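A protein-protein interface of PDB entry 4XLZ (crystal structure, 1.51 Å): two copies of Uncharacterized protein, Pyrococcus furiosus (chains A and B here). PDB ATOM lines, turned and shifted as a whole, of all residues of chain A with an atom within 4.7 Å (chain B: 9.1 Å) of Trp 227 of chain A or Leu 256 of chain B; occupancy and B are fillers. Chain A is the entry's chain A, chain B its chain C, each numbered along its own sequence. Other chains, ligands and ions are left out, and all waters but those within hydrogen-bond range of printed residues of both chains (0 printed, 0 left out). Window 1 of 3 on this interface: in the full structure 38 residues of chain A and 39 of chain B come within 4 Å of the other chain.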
ATOM      1  N   ILE A  46      -6.519 -24.674 -10.707  1.00  0.00           N
ATOM      2  CA  ILE A  46      -5.681 -23.996 -11.773  1.00  0.00           C
ATOM      3  C   ILE A  46      -4.623 -23.152 -11.192  1.00  0.00           C
ATOM      4  O   ILE A  46      -3.434 -23.192 -11.615  1.00  0.00           O
ATOM      5  CB  ILE A  46      -6.576 -23.261 -12.759  1.00  0.00           C
ATOM      6  CG1 ILE A  46      -7.564 -24.162 -13.488  1.00  0.00           C
ATOM      7  CG2 ILE A  46      -5.734 -22.314 -13.717  1.00  0.00           C
ATOM      8  CD1 ILE A  46      -8.704 -23.412 -14.202  1.00  0.00           C
ATOM      9  N   PHE A 219     -13.425 -28.069 -19.529  1.00  0.00           N
ATOM     10  CA  PHE A 219     -12.113 -28.462 -20.315  1.00  0.00           C
ATOM     11  C   PHE A 219     -12.478 -29.619 -21.186  1.00  0.00           C
ATOM     12  O   PHE A 219     -12.094 -30.785 -20.845  1.00  0.00           O
ATOM     13  CB  PHE A 219     -11.008 -28.764 -19.303  1.00  0.00           C
ATOM     14  CG  PHE A 219     -10.591 -27.499 -18.561  1.00  0.00           C
ATOM     15  CD1 PHE A 219      -9.983 -26.455 -19.305  1.00  0.00           C
ATOM     16  CD2 PHE A 219     -10.915 -27.344 -17.224  1.00  0.00           C
ATOM     17  CE1 PHE A 219      -9.671 -25.237 -18.685  1.00  0.00           C
ATOM     18  CE2 PHE A 219     -10.544 -26.119 -16.546  1.00  0.00           C
ATOM     19  CZ  PHE A 219     -10.002 -25.047 -17.268  1.00  0.00           C
ATOM     20  N   ILE A 223     -11.105 -27.401 -25.955  1.00  0.00           N
ATOM     21  CA  ILE A 223     -10.609 -26.277 -25.167  1.00  0.00           C
ATOM     22  C   ILE A 223      -9.220 -26.567 -24.610  1.00  0.00           C
ATOM     23  O   ILE A 223      -8.355 -25.733 -24.504  1.00  0.00           O
ATOM     24  CB  ILE A 223     -11.641 -25.981 -23.984  1.00  0.00           C
ATOM     25  CG1 ILE A 223     -12.843 -25.340 -24.672  1.00  0.00           C
ATOM     26  CG2 ILE A 223     -10.973 -25.145 -22.901  1.00  0.00           C
ATOM     27  CD1 ILE A 223     -14.042 -25.141 -23.666  1.00  0.00           C
ATOM     28  N   TRP A 224      -8.978 -27.881 -24.306  1.00  0.00           N
ATOM     29  CA  TRP A 224      -7.739 -28.288 -23.721  1.00  0.00           C
ATOM     30  C   TRP A 224      -6.541 -28.099 -24.704  1.00  0.00           C
ATOM     31  O   TRP A 224      -5.424 -27.925 -24.236  1.00  0.00           O
ATOM     32  CB  TRP A 224      -7.873 -29.765 -23.229  1.00  0.00           C
ATOM     33  CG  TRP A 224      -6.757 -30.147 -22.264  1.00  0.00           C
ATOM     34  CD1 TRP A 224      -5.738 -31.120 -22.423  1.00  0.00           C
ATOM     35  CD2 TRP A 224      -6.549 -29.630 -20.944  1.00  0.00           C
ATOM     36  NE1 TRP A 224      -4.941 -31.178 -21.302  1.00  0.00           N
ATOM     37  CE2 TRP A 224      -5.409 -30.285 -20.362  1.00  0.00           C
ATOM     38  CE3 TRP A 224      -7.247 -28.643 -20.196  1.00  0.00           C
ATOM     39  CZ2 TRP A 224      -4.943 -30.016 -19.070  1.00  0.00           C
ATOM     40  CZ3 TRP A 224      -6.801 -28.380 -18.897  1.00  0.00           C
ATOM     41  CH2 TRP A 224      -5.637 -29.019 -18.361  1.00  0.00           C
ATOM     42  N   GLU A 225      -6.892 -28.133 -26.023  1.00  0.00           N
ATOM     43  CA  GLU A 225      -5.801 -27.840 -26.965  1.00  0.00           C
ATOM     44  C   GLU A 225      -5.185 -26.467 -26.839  1.00  0.00           C
ATOM     45  O   GLU A 225      -4.044 -26.244 -27.222  1.00  0.00           O
ATOM     46  CB  GLU A 225      -6.333 -27.951 -28.381  1.00  0.00           C
ATOM     47  CG  GLU A 225      -6.763 -29.435 -28.751  1.00  0.00           C
ATOM     48  CD  GLU A 225      -5.557 -30.442 -28.623  1.00  0.00           C
ATOM     49  OE1 GLU A 225      -5.477 -31.246 -27.688  1.00  0.00           O
ATOM     50  OE2 GLU A 225      -4.667 -30.281 -29.553  1.00  0.00           O
ATOM     51  N   THR A 226      -5.933 -25.518 -26.214  1.00  0.00           N
ATOM     52  CA  THR A 226      -5.335 -24.238 -25.891  1.00  0.00           C
ATOM     53  C   THR A 226      -4.917 -24.139 -24.476  1.00  0.00           C
ATOM     54  O   THR A 226      -3.889 -23.621 -24.109  1.00  0.00           O
ATOM     55  CB  THR A 226      -6.430 -23.124 -26.153  1.00  0.00           C
ATOM     56  OG1 THR A 226      -6.709 -23.045 -27.579  1.00  0.00           O
ATOM     57  CG2 THR A 226      -5.901 -21.772 -25.621  1.00  0.00           C
ATOM     58  N   TRP A 227      -5.729 -24.776 -23.596  1.00  0.00           N
ATOM     59  CA  TRP A 227      -5.393 -24.637 -22.171  1.00  0.00           C
ATOM     60  C   TRP A 227      -4.233 -25.375 -21.618  1.00  0.00           C
ATOM     61  O   TRP A 227      -3.471 -24.962 -20.746  1.00  0.00           O
ATOM     62  CB  TRP A 227      -6.649 -24.914 -21.281  1.00  0.00           C
ATOM     63  CG  TRP A 227      -7.463 -23.593 -21.295  1.00  0.00           C
ATOM     64  CD1 TRP A 227      -8.192 -23.050 -22.370  1.00  0.00           C
ATOM     65  CD2 TRP A 227      -7.561 -22.629 -20.226  1.00  0.00           C
ATOM     66  NE1 TRP A 227      -8.700 -21.770 -22.013  1.00  0.00           N
ATOM     67  CE2 TRP A 227      -8.308 -21.523 -20.726  1.00  0.00           C
ATOM     68  CE3 TRP A 227      -7.051 -22.593 -18.926  1.00  0.00           C
ATOM     69  CZ2 TRP A 227      -8.661 -20.397 -19.903  1.00  0.00           C
ATOM     70  CZ3 TRP A 227      -7.408 -21.486 -18.089  1.00  0.00           C
ATOM     71  CH2 TRP A 227      -8.156 -20.396 -18.613  1.00  0.00           C
ATOM     72  N   GLU A 228      -3.924 -26.595 -22.159  1.00  0.00           N
ATOM     73  CA  GLU A 228      -2.650 -27.262 -21.729  1.00  0.00           C
ATOM     74  C   GLU A 228      -1.435 -26.435 -22.071  1.00  0.00           C
ATOM     75  O   GLU A 228      -0.600 -26.194 -21.228  1.00  0.00           O
ATOM     76  CB  GLU A 228      -2.573 -28.817 -22.133  1.00  0.00           C
ATOM     77  CG  GLU A 228      -1.365 -29.402 -21.516  1.00  0.00           C
ATOM     78  CD  GLU A 228      -1.166 -30.894 -21.754  1.00  0.00           C
ATOM     79  OE1 GLU A 228      -0.040 -31.334 -21.585  1.00  0.00           O
ATOM     80  OE2 GLU A 228      -2.148 -31.606 -21.976  1.00  0.00           O
ATOM     81  N   PRO A 229      -1.343 -25.937 -23.302  1.00  0.00           N
ATOM     82  CA  PRO A 229      -0.195 -25.041 -23.614  1.00  0.00           C
ATOM     83  C   PRO A 229      -0.178 -23.764 -22.687  1.00  0.00           C
ATOM     84  O   PRO A 229       0.896 -23.426 -22.200  1.00  0.00           O
ATOM     85  CB  PRO A 229      -0.513 -24.610 -25.055  1.00  0.00           C
ATOM     86  CG  PRO A 229      -1.149 -25.892 -25.730  1.00  0.00           C
ATOM     87  CD  PRO A 229      -2.091 -26.409 -24.542  1.00  0.00           C
ATOM     88  N   PHE A 230      -1.373 -23.206 -22.483  1.00  0.00           N
ATOM     89  CA  PHE A 230      -1.393 -22.017 -21.578  1.00  0.00           C
ATOM     90  C   PHE A 230      -0.902 -22.384 -20.216  1.00  0.00           C
ATOM     91  O   PHE A 230      -0.025 -21.674 -19.610  1.00  0.00           O
ATOM     92  CB  PHE A 230      -2.857 -21.500 -21.588  1.00  0.00           C
ATOM     93  CG  PHE A 230      -3.080 -20.347 -20.628  1.00  0.00           C
ATOM     94  CD1 PHE A 230      -2.338 -19.198 -20.744  1.00  0.00           C
ATOM     95  CD2 PHE A 230      -4.006 -20.432 -19.611  1.00  0.00           C
ATOM     96  CE1 PHE A 230      -2.545 -18.018 -19.854  1.00  0.00           C
ATOM     97  CE2 PHE A 230      -4.208 -19.293 -18.731  1.00  0.00           C
ATOM     98  CZ  PHE A 230      -3.490 -18.122 -18.924  1.00  0.00           C
ATOM     99  N   LEU A 231      -1.413 -23.460 -19.621  1.00  0.00           N
ATOM    100  CA  LEU A 231      -1.035 -23.805 -18.268  1.00  0.00           C
ATOM    101  C   LEU A 231       0.431 -24.179 -18.145  1.00  0.00           C
ATOM    102  O   LEU A 231       1.107 -23.839 -17.197  1.00  0.00           O
ATOM    103  CB  LEU A 231      -1.827 -25.043 -17.770  1.00  0.00           C
ATOM    104  CG  LEU A 231      -3.329 -24.690 -17.610  1.00  0.00           C
ATOM    105  CD1 LEU A 231      -4.202 -25.981 -17.444  1.00  0.00           C
ATOM    106  CD2 LEU A 231      -3.592 -23.854 -16.371  1.00  0.00           C
ATOM    107  N   MET B   1       1.213 -31.829 -24.292  1.00  0.00           N
ATOM    108  CA  MET B   1       1.510 -30.712 -25.149  1.00  0.00           C
ATOM    109  C   MET B   1       2.394 -29.736 -24.479  1.00  0.00           C
ATOM    110  O   MET B   1       2.365 -29.596 -23.248  1.00  0.00           O
ATOM    111  CB  MET B   1       0.212 -30.008 -25.496  1.00  0.00           C
ATOM    112  CG  MET B   1      -0.670 -30.877 -26.400  1.00  0.00           C
ATOM    113  SD  MET B   1      -2.412 -30.124 -26.767  1.00  0.00           S
ATOM    114  CE  MET B   1      -3.341 -30.832 -25.168  1.00  0.00           C
ATOM    115  N   PHE B   2       3.180 -28.988 -25.272  1.00  0.00           N
ATOM    116  CA  PHE B   2       4.129 -28.031 -24.706  1.00  0.00           C
ATOM    117  C   PHE B   2       5.116 -28.588 -23.737  1.00  0.00           C
ATOM    118  O   PHE B   2       5.679 -27.931 -22.844  1.00  0.00           O
ATOM    119  CB  PHE B   2       3.378 -26.795 -24.075  1.00  0.00           C
ATOM    120  CG  PHE B   2       3.129 -25.698 -25.063  1.00  0.00           C
ATOM    121  CD1 PHE B   2       3.498 -24.377 -24.730  1.00  0.00           C
ATOM    122  CD2 PHE B   2       2.535 -25.891 -26.337  1.00  0.00           C
ATOM    123  CE1 PHE B   2       3.247 -23.329 -25.522  1.00  0.00           C
ATOM    124  CE2 PHE B   2       2.289 -24.808 -27.226  1.00  0.00           C
ATOM    125  CZ  PHE B   2       2.687 -23.454 -26.753  1.00  0.00           C
ATOM    126  N   LEU B  15       3.117 -20.119 -27.785  1.00  0.00           N
ATOM    127  CA  LEU B  15       1.717 -19.875 -27.384  1.00  0.00           C
ATOM    128  C   LEU B  15       1.135 -18.775 -28.265  1.00  0.00           C
ATOM    129  O   LEU B  15       0.002 -18.915 -28.724  1.00  0.00           O
ATOM    130  CB  LEU B  15       1.699 -19.540 -25.845  1.00  0.00           C
ATOM    131  CG  LEU B  15       0.221 -19.234 -25.397  1.00  0.00           C
ATOM    132  CD1 LEU B  15      -0.562 -20.559 -25.201  1.00  0.00           C
ATOM    133  CD2 LEU B  15       0.392 -18.552 -24.012  1.00  0.00           C
ATOM    134  N   LEU B  16       1.840 -17.667 -28.415  1.00  0.00           N
ATOM    135  CA  LEU B  16       1.278 -16.560 -29.192  1.00  0.00           C
ATOM    136  C   LEU B  16       1.194 -16.830 -30.651  1.00  0.00           C
ATOM    137  O   LEU B  16       0.155 -16.593 -31.238  1.00  0.00           O
ATOM    138  CB  LEU B  16       2.174 -15.329 -28.953  1.00  0.00           C
ATOM    139  CG  LEU B  16       1.927 -14.474 -27.750  1.00  0.00           C
ATOM    140  CD1 LEU B  16       3.025 -13.384 -27.990  1.00  0.00           C
ATOM    141  CD2 LEU B  16       0.561 -13.797 -27.779  1.00  0.00           C
ATOM    142  N   VAL B  19      -0.427 -21.349 -30.986  1.00  0.00           N
ATOM    143  CA  VAL B  19      -1.689 -21.740 -30.362  1.00  0.00           C
ATOM    144  C   VAL B  19      -2.810 -20.627 -30.515  1.00  0.00           C
ATOM    145  O   VAL B  19      -3.961 -20.938 -30.834  1.00  0.00           O
ATOM    146  CB  VAL B  19      -1.448 -22.001 -28.868  1.00  0.00           C
ATOM    147  CG1 VAL B  19      -2.762 -22.237 -28.064  1.00  0.00           C
ATOM    148  CG2 VAL B  19      -0.389 -23.175 -28.628  1.00  0.00           C
ATOM    149  N   LEU B  20      -2.417 -19.366 -30.318  1.00  0.00           N
ATOM    150  CA  LEU B  20      -3.378 -18.245 -30.290  1.00  0.00           C
ATOM    151  C   LEU B  20      -3.409 -17.540 -31.660  1.00  0.00           C
ATOM    152  O   LEU B  20      -4.347 -16.755 -31.932  1.00  0.00           O
ATOM    153  CB  LEU B  20      -2.968 -17.303 -29.146  1.00  0.00           C
ATOM    154  CG  LEU B  20      -3.008 -17.899 -27.768  1.00  0.00           C
ATOM    155  CD1 LEU B  20      -2.559 -16.828 -26.762  1.00  0.00           C
ATOM    156  CD2 LEU B  20      -4.426 -18.397 -27.513  1.00  0.00           C
ATOM    157  N   PHE B  22      -1.764 -15.222 -32.897  1.00  0.00           N
ATOM    158  CA  PHE B  22      -1.845 -13.787 -32.693  1.00  0.00           C
ATOM    159  C   PHE B  22      -0.812 -13.048 -33.576  1.00  0.00           C
ATOM    160  O   PHE B  22       0.368 -13.315 -33.520  1.00  0.00           O
ATOM    161  CB  PHE B  22      -1.577 -13.503 -31.205  1.00  0.00           C
ATOM    162  CG  PHE B  22      -1.679 -12.037 -30.854  1.00  0.00           C
ATOM    163  CD1 PHE B  22      -2.947 -11.477 -30.846  1.00  0.00           C
ATOM    164  CD2 PHE B  22      -0.545 -11.365 -30.483  1.00  0.00           C
ATOM    165  CE1 PHE B  22      -3.053 -10.103 -30.457  1.00  0.00           C
ATOM    166  CE2 PHE B  22      -0.656  -9.993 -30.124  1.00  0.00           C
ATOM    167  CZ  PHE B  22      -1.969  -9.476 -30.100  1.00  0.00           C
ATOM    168  N   ILE B 187     -11.004  -7.351 -30.067  1.00  0.00           N
ATOM    169  CA  ILE B 187     -11.242  -6.054 -29.325  1.00  0.00           C
ATOM    170  C   ILE B 187      -9.953  -5.206 -29.615  1.00  0.00           C
ATOM    171  O   ILE B 187      -8.814  -5.715 -29.611  1.00  0.00           O
ATOM    172  CB  ILE B 187     -11.263  -6.389 -27.859  1.00  0.00           C
ATOM    173  CG1 ILE B 187     -12.599  -7.041 -27.584  1.00  0.00           C
ATOM    174  CG2 ILE B 187     -11.275  -5.062 -27.022  1.00  0.00           C
ATOM    175  CD1 ILE B 187     -12.527  -7.599 -26.063  1.00  0.00           C
ATOM    176  N   MET B 253      -4.968  -7.709 -27.838  1.00  0.00           N
ATOM    177  CA  MET B 253      -4.327  -8.871 -27.212  1.00  0.00           C
ATOM    178  C   MET B 253      -5.222 -10.080 -27.573  1.00  0.00           C
ATOM    179  O   MET B 253      -6.404  -9.950 -27.850  1.00  0.00           O
ATOM    180  CB  MET B 253      -4.437  -8.792 -25.648  1.00  0.00           C
ATOM    181  CG  MET B 253      -3.679  -7.515 -25.117  1.00  0.00           C
ATOM    182  SD  MET B 253      -3.449  -7.661 -23.149  1.00  0.00           S
ATOM    183  CE  MET B 253      -5.371  -7.505 -22.659  1.00  0.00           C
ATOM    184  N   PRO B 254      -4.664 -11.278 -27.463  1.00  0.00           N
ATOM    185  CA  PRO B 254      -5.454 -12.483 -27.590  1.00  0.00           C
ATOM    186  C   PRO B 254      -6.545 -12.434 -26.485  1.00  0.00           C
ATOM    187  O   PRO B 254      -6.302 -11.951 -25.361  1.00  0.00           O
ATOM    188  CB  PRO B 254      -4.474 -13.597 -27.203  1.00  0.00           C
ATOM    189  CG  PRO B 254      -3.125 -13.090 -27.510  1.00  0.00           C
ATOM    190  CD  PRO B 254      -3.259 -11.548 -27.181  1.00  0.00           C
ATOM    191  N   GLY B 255      -7.698 -13.017 -26.792  1.00  0.00           N
ATOM    192  CA  GLY B 255      -8.802 -13.044 -25.742  1.00  0.00           C
ATOM    193  C   GLY B 255      -8.289 -13.640 -24.483  1.00  0.00           C
ATOM    194  O   GLY B 255      -8.704 -13.181 -23.347  1.00  0.00           O
ATOM    195  N   LEU B 256      -7.508 -14.720 -24.522  1.00  0.00           N
ATOM    196  CA  LEU B 256      -7.028 -15.386 -23.344  1.00  0.00           C
ATOM    197  C   LEU B 256      -6.317 -14.432 -22.395  1.00  0.00           C
ATOM    198  O   LEU B 256      -6.355 -14.600 -21.176  1.00  0.00           O
ATOM    199  CB  LEU B 256      -5.966 -16.458 -23.835  1.00  0.00           C
ATOM    200  CG  LEU B 256      -5.536 -17.489 -22.839  1.00  0.00           C
ATOM    201  CD1 LEU B 256      -6.677 -18.471 -22.583  1.00  0.00           C
ATOM    202  CD2 LEU B 256      -4.349 -18.321 -23.537  1.00  0.00           C
ATOM    203  N   PHE B 257      -5.628 -13.405 -22.920  1.00  0.00           N
ATOM    204  CA  PHE B 257      -4.755 -12.611 -22.086  1.00  0.00           C
ATOM    205  C   PHE B 257      -5.538 -11.601 -21.203  1.00  0.00           C
ATOM    206  O   PHE B 257      -4.886 -11.034 -20.334  1.00  0.00           O
ATOM    207  CB  PHE B 257      -3.795 -11.762 -22.949  1.00  0.00           C
ATOM    208  CG  PHE B 257      -2.521 -12.525 -23.371  1.00  0.00           C
ATOM    209  CD1 PHE B 257      -2.531 -13.912 -23.558  1.00  0.00           C
ATOM    210  CD2 PHE B 257      -1.324 -11.794 -23.573  1.00  0.00           C
ATOM    211  CE1 PHE B 257      -1.334 -14.593 -23.949  1.00  0.00           C
ATOM    212  CE2 PHE B 257      -0.134 -12.457 -23.942  1.00  0.00           C
ATOM    213  CZ  PHE B 257      -0.172 -13.876 -24.120  1.00  0.00           C
ATOM    214  N   TYR B 258      -6.852 -11.487 -21.439  1.00  0.00           N
ATOM    215  CA  TYR B 258      -7.685 -10.650 -20.533  1.00  0.00           C
ATOM    216  C   TYR B 258      -8.036 -11.420 -19.303  1.00  0.00           C
ATOM    217  O   TYR B 258      -8.921 -10.889 -18.532  1.00  0.00           O
ATOM    218  CB  TYR B 258      -8.964 -10.267 -21.306  1.00  0.00           C
ATOM    219  CG  TYR B 258      -8.770  -9.260 -22.425  1.00  0.00           C
ATOM    220  CD1 TYR B 258      -8.960  -7.951 -22.150  1.00  0.00           C
ATOM    221  CD2 TYR B 258      -8.401  -9.725 -23.736  1.00  0.00           C
ATOM    222  CE1 TYR B 258      -8.728  -7.000 -23.190  1.00  0.00           C
ATOM    223  CE2 TYR B 258      -8.254  -8.735 -24.777  1.00  0.00           C
ATOM    224  CZ  TYR B 258      -8.425  -7.459 -24.455  1.00  0.00           C
ATOM    225  OH  TYR B 258      -8.345  -6.499 -25.512  1.00  0.00           O
ATOM    226  N   HIS B 259      -7.392 -12.548 -18.997  1.00  0.00           N
ATOM    227  CA  HIS B 259      -7.861 -13.292 -17.792  1.00  0.00           C
ATOM    228  C   HIS B 259      -6.746 -14.167 -17.298  1.00  0.00           C
ATOM    229  O   HIS B 259      -6.161 -14.925 -18.139  1.00  0.00           O
ATOM    230  CB  HIS B 259      -9.080 -14.062 -18.199  1.00  0.00           C
ATOM    231  CG  HIS B 259      -9.752 -14.822 -17.094  1.00  0.00           C
ATOM    232  ND1 HIS B 259     -10.134 -14.193 -15.914  1.00  0.00           N
ATOM    233  CD2 HIS B 259     -10.141 -16.132 -16.980  1.00  0.00           C
ATOM    234  CE1 HIS B 259     -10.848 -15.074 -15.171  1.00  0.00           C
ATOM    235  NE2 HIS B 259     -10.824 -16.268 -15.773  1.00  0.00           N
ATOM    236  N   ILE B 260      -6.455 -14.111 -16.014  1.00  0.00           N
ATOM    237  CA  ILE B 260      -5.467 -14.983 -15.367  1.00  0.00           C
ATOM    238  C   ILE B 260      -4.123 -15.146 -16.133  1.00  0.00           C
ATOM    239  O   ILE B 260      -3.492 -16.221 -16.047  1.00  0.00           O
ATOM    240  CB  ILE B 260      -6.052 -16.343 -14.925  1.00  0.00           C
ATOM    241  CG1 ILE B 260      -6.445 -17.252 -16.078  1.00  0.00           C
ATOM    242  CG2 ILE B 260      -7.243 -16.169 -13.968  1.00  0.00           C
ATOM    243  CD1 ILE B 260      -6.644 -18.749 -15.560  1.00  0.00           C
ATOM    244  N   THR B 261      -3.627 -14.095 -16.793  1.00  0.00           N
ATOM    245  CA  THR B 261      -2.413 -14.282 -17.629  1.00  0.00           C
ATOM    246  C   THR B 261      -1.336 -13.384 -16.972  1.00  0.00           C
ATOM    247  O   THR B 261      -1.323 -12.139 -17.177  1.00  0.00           O
ATOM    248  CB  THR B 261      -2.743 -13.830 -19.059  1.00  0.00           C
ATOM    249  OG1 THR B 261      -3.639 -14.721 -19.654  1.00  0.00           O
ATOM    250  CG2 THR B 261      -1.406 -13.914 -19.891  1.00  0.00           C
ATOM    251  N   PRO B 262      -0.344 -13.990 -16.344  1.00  0.00           N
ATOM    252  CA  PRO B 262       0.630 -13.176 -15.587  1.00  0.00           C
ATOM    253  C   PRO B 262       1.672 -12.483 -16.441  1.00  0.00           C
ATOM    254  O   PRO B 262       2.397 -11.668 -15.944  1.00  0.00           O
ATOM    255  CB  PRO B 262       1.309 -14.137 -14.584  1.00  0.00           C
ATOM    256  CG  PRO B 262       1.043 -15.484 -15.240  1.00  0.00           C
ATOM    257  CD  PRO B 262      -0.241 -15.418 -16.050  1.00  0.00           C
ATOM    258  N   PHE B 263       1.691 -12.759 -17.732  1.00  0.00           N
ATOM    259  CA  PHE B 263       2.657 -12.092 -18.632  1.00  0.00           C
ATOM    260  C   PHE B 263       1.944 -11.358 -19.749  1.00  0.00           C
ATOM    261  O   PHE B 263       2.513 -11.109 -20.837  1.00  0.00           O
ATOM    262  CB  PHE B 263       3.598 -13.203 -19.259  1.00  0.00           C
ATOM    263  CG  PHE B 263       2.849 -14.482 -19.660  1.00  0.00           C
ATOM    264  CD1 PHE B 263       2.945 -15.649 -18.883  1.00  0.00           C
ATOM    265  CD2 PHE B 263       2.039 -14.588 -20.821  1.00  0.00           C
ATOM    266  CE1 PHE B 263       2.255 -16.816 -19.329  1.00  0.00           C
ATOM    267  CE2 PHE B 263       1.352 -15.721 -21.203  1.00  0.00           C
ATOM    268  CZ  PHE B 263       1.455 -16.825 -20.426  1.00  0.00           C
ATOM    269  N   ALA B 264       0.682 -10.904 -19.481  1.00  0.00           N
ATOM    270  CA  ALA B 264      -0.012 -10.126 -20.446  1.00  0.00           C
ATOM    271  C   ALA B 264       0.703  -8.796 -20.764  1.00  0.00           C
ATOM    272  O   ALA B 264       0.449  -8.308 -21.918  1.00  0.00           O
ATOM    273  CB  ALA B 264      -1.520  -9.900 -19.941  1.00  0.00           C
ATOM    274  N   ILE B 267       3.184  -8.215 -24.189  1.00  0.00           N
ATOM    275  CA  ILE B 267       2.809  -7.667 -25.500  1.00  0.00           C
ATOM    276  C   ILE B 267       2.332  -6.233 -25.443  1.00  0.00           C
ATOM    277  O   ILE B 267       2.121  -5.628 -26.520  1.00  0.00           O
ATOM    278  CB  ILE B 267       1.784  -8.580 -26.242  1.00  0.00           C
ATOM    279  CG1 ILE B 267       0.442  -8.698 -25.460  1.00  0.00           C
ATOM    280  CG2 ILE B 267       2.410  -9.995 -26.489  1.00  0.00           C
ATOM    281  CD1 ILE B 267      -0.632  -9.440 -26.272  1.00  0.00           C
ATOM    282  OXT ILE B 267       2.125  -5.715 -24.339  1.00  0.00           O
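The side-chain carboxylate (OE1) of Glu 228 of chain A sits at hydrogen-bond distance from the backbone NH (N) of Met 1 of chain B (3.0 Å).
OE1 of Glu 225 of chain A sits close to SD of Met 1 of chain B (3.4 Å).
The indole nitrogen (NE1) of Trp 224 of chain A lies within hydrogen-bond range of the side-chain carboxylate (OE2) of Glu 228 of chain A, 2.9 Å away.
The backbone NH (N) of Leu 20 of chain B sits at hydrogen-bond distance from the backbone carbonyl oxygen (O) of Leu 15 of chain B (2.9 Å).
The backbone carbonyl oxygen of Leu 256 of chain B is in hydrogen-bond range of the side-chain hydroxyl of Thr 261 of chain B, at 3.1 Å.
The backbone carbonyl oxygen (O) of His 259 of chain B lies within hydrogen-bond range of the side-chain hydroxyl (OG1) of Thr 261 of chain B (2.9 Å).
CD1 of Trp 224 of chain A touches CE of Met 1 of chain B, at 3.7 Å.
Thr 226 of chain A touches Val 19 of chain B (CA to CG1, 3.9 Å).
Trp 227 of chain A touches Leu 256 of chain B.
Trp 227 of chain A touches Ile 260 of chain B (CH2 to CD1, 3.8 Å).
Pro 229 of chain A touches Phe 2 of chain B (CB to CD2, 3.5 Å).
Val 19 of chain B touches Pro 229 of chain A.
Phe 230 of chain A touches Leu 15 of chain B.
Leu 256 of chain B touches Phe 230 of chain A.
CZ of Phe 230 of chain A touches O of Ile 260 of chain B (3.4 Å).
Phe 230 of chain A touches Thr 261 of chain B (CE1 to OG1, 3.5 Å).
Thr 226 of chain A touches just one residue of chain B: Val 19 (3.9 Å).
Printed residues of chain B within 4 Å of Trp 227 of chain A: Leu 256 and Ile 260.
Of the printed residues of chain B, Glu 228 of chain A touches Met 1 (3.0 Å).
Of the printed residues of chain A, Leu 15 of chain B touches Phe 230 (3.9 Å).
Of the printed residues of chain A, Val 19 of chain B touches Thr 226 and Pro 229.
Ile 187 of chain B touches none of the printed residues of chain A.
Of the printed residues of chain A, Leu 256 of chain B touches Trp 227 and Phe 230.
Of the printed residues of chain A, Ile 260 of chain B touches Trp 227 and Phe 230.
The nearest residue of chain B that does not touch Trp 227 of chain A is His 259 of chain B (5.0 Å).
Of the 11 printed residues of chain A, 7 touch a printed residue of chain B.
Hydrophobic or aromatic side chains of chain B within 4 Å of the printed part of chain A: Met 1, Phe 2, Leu 15, Val 19, Leu 256 and Ile 260.
Along chain B the printed residues that touch a printed residue of chain A span positions 1 to 261.
Among the printed residues, 12 pairs touch across the chains.
No position is printed for both chains.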
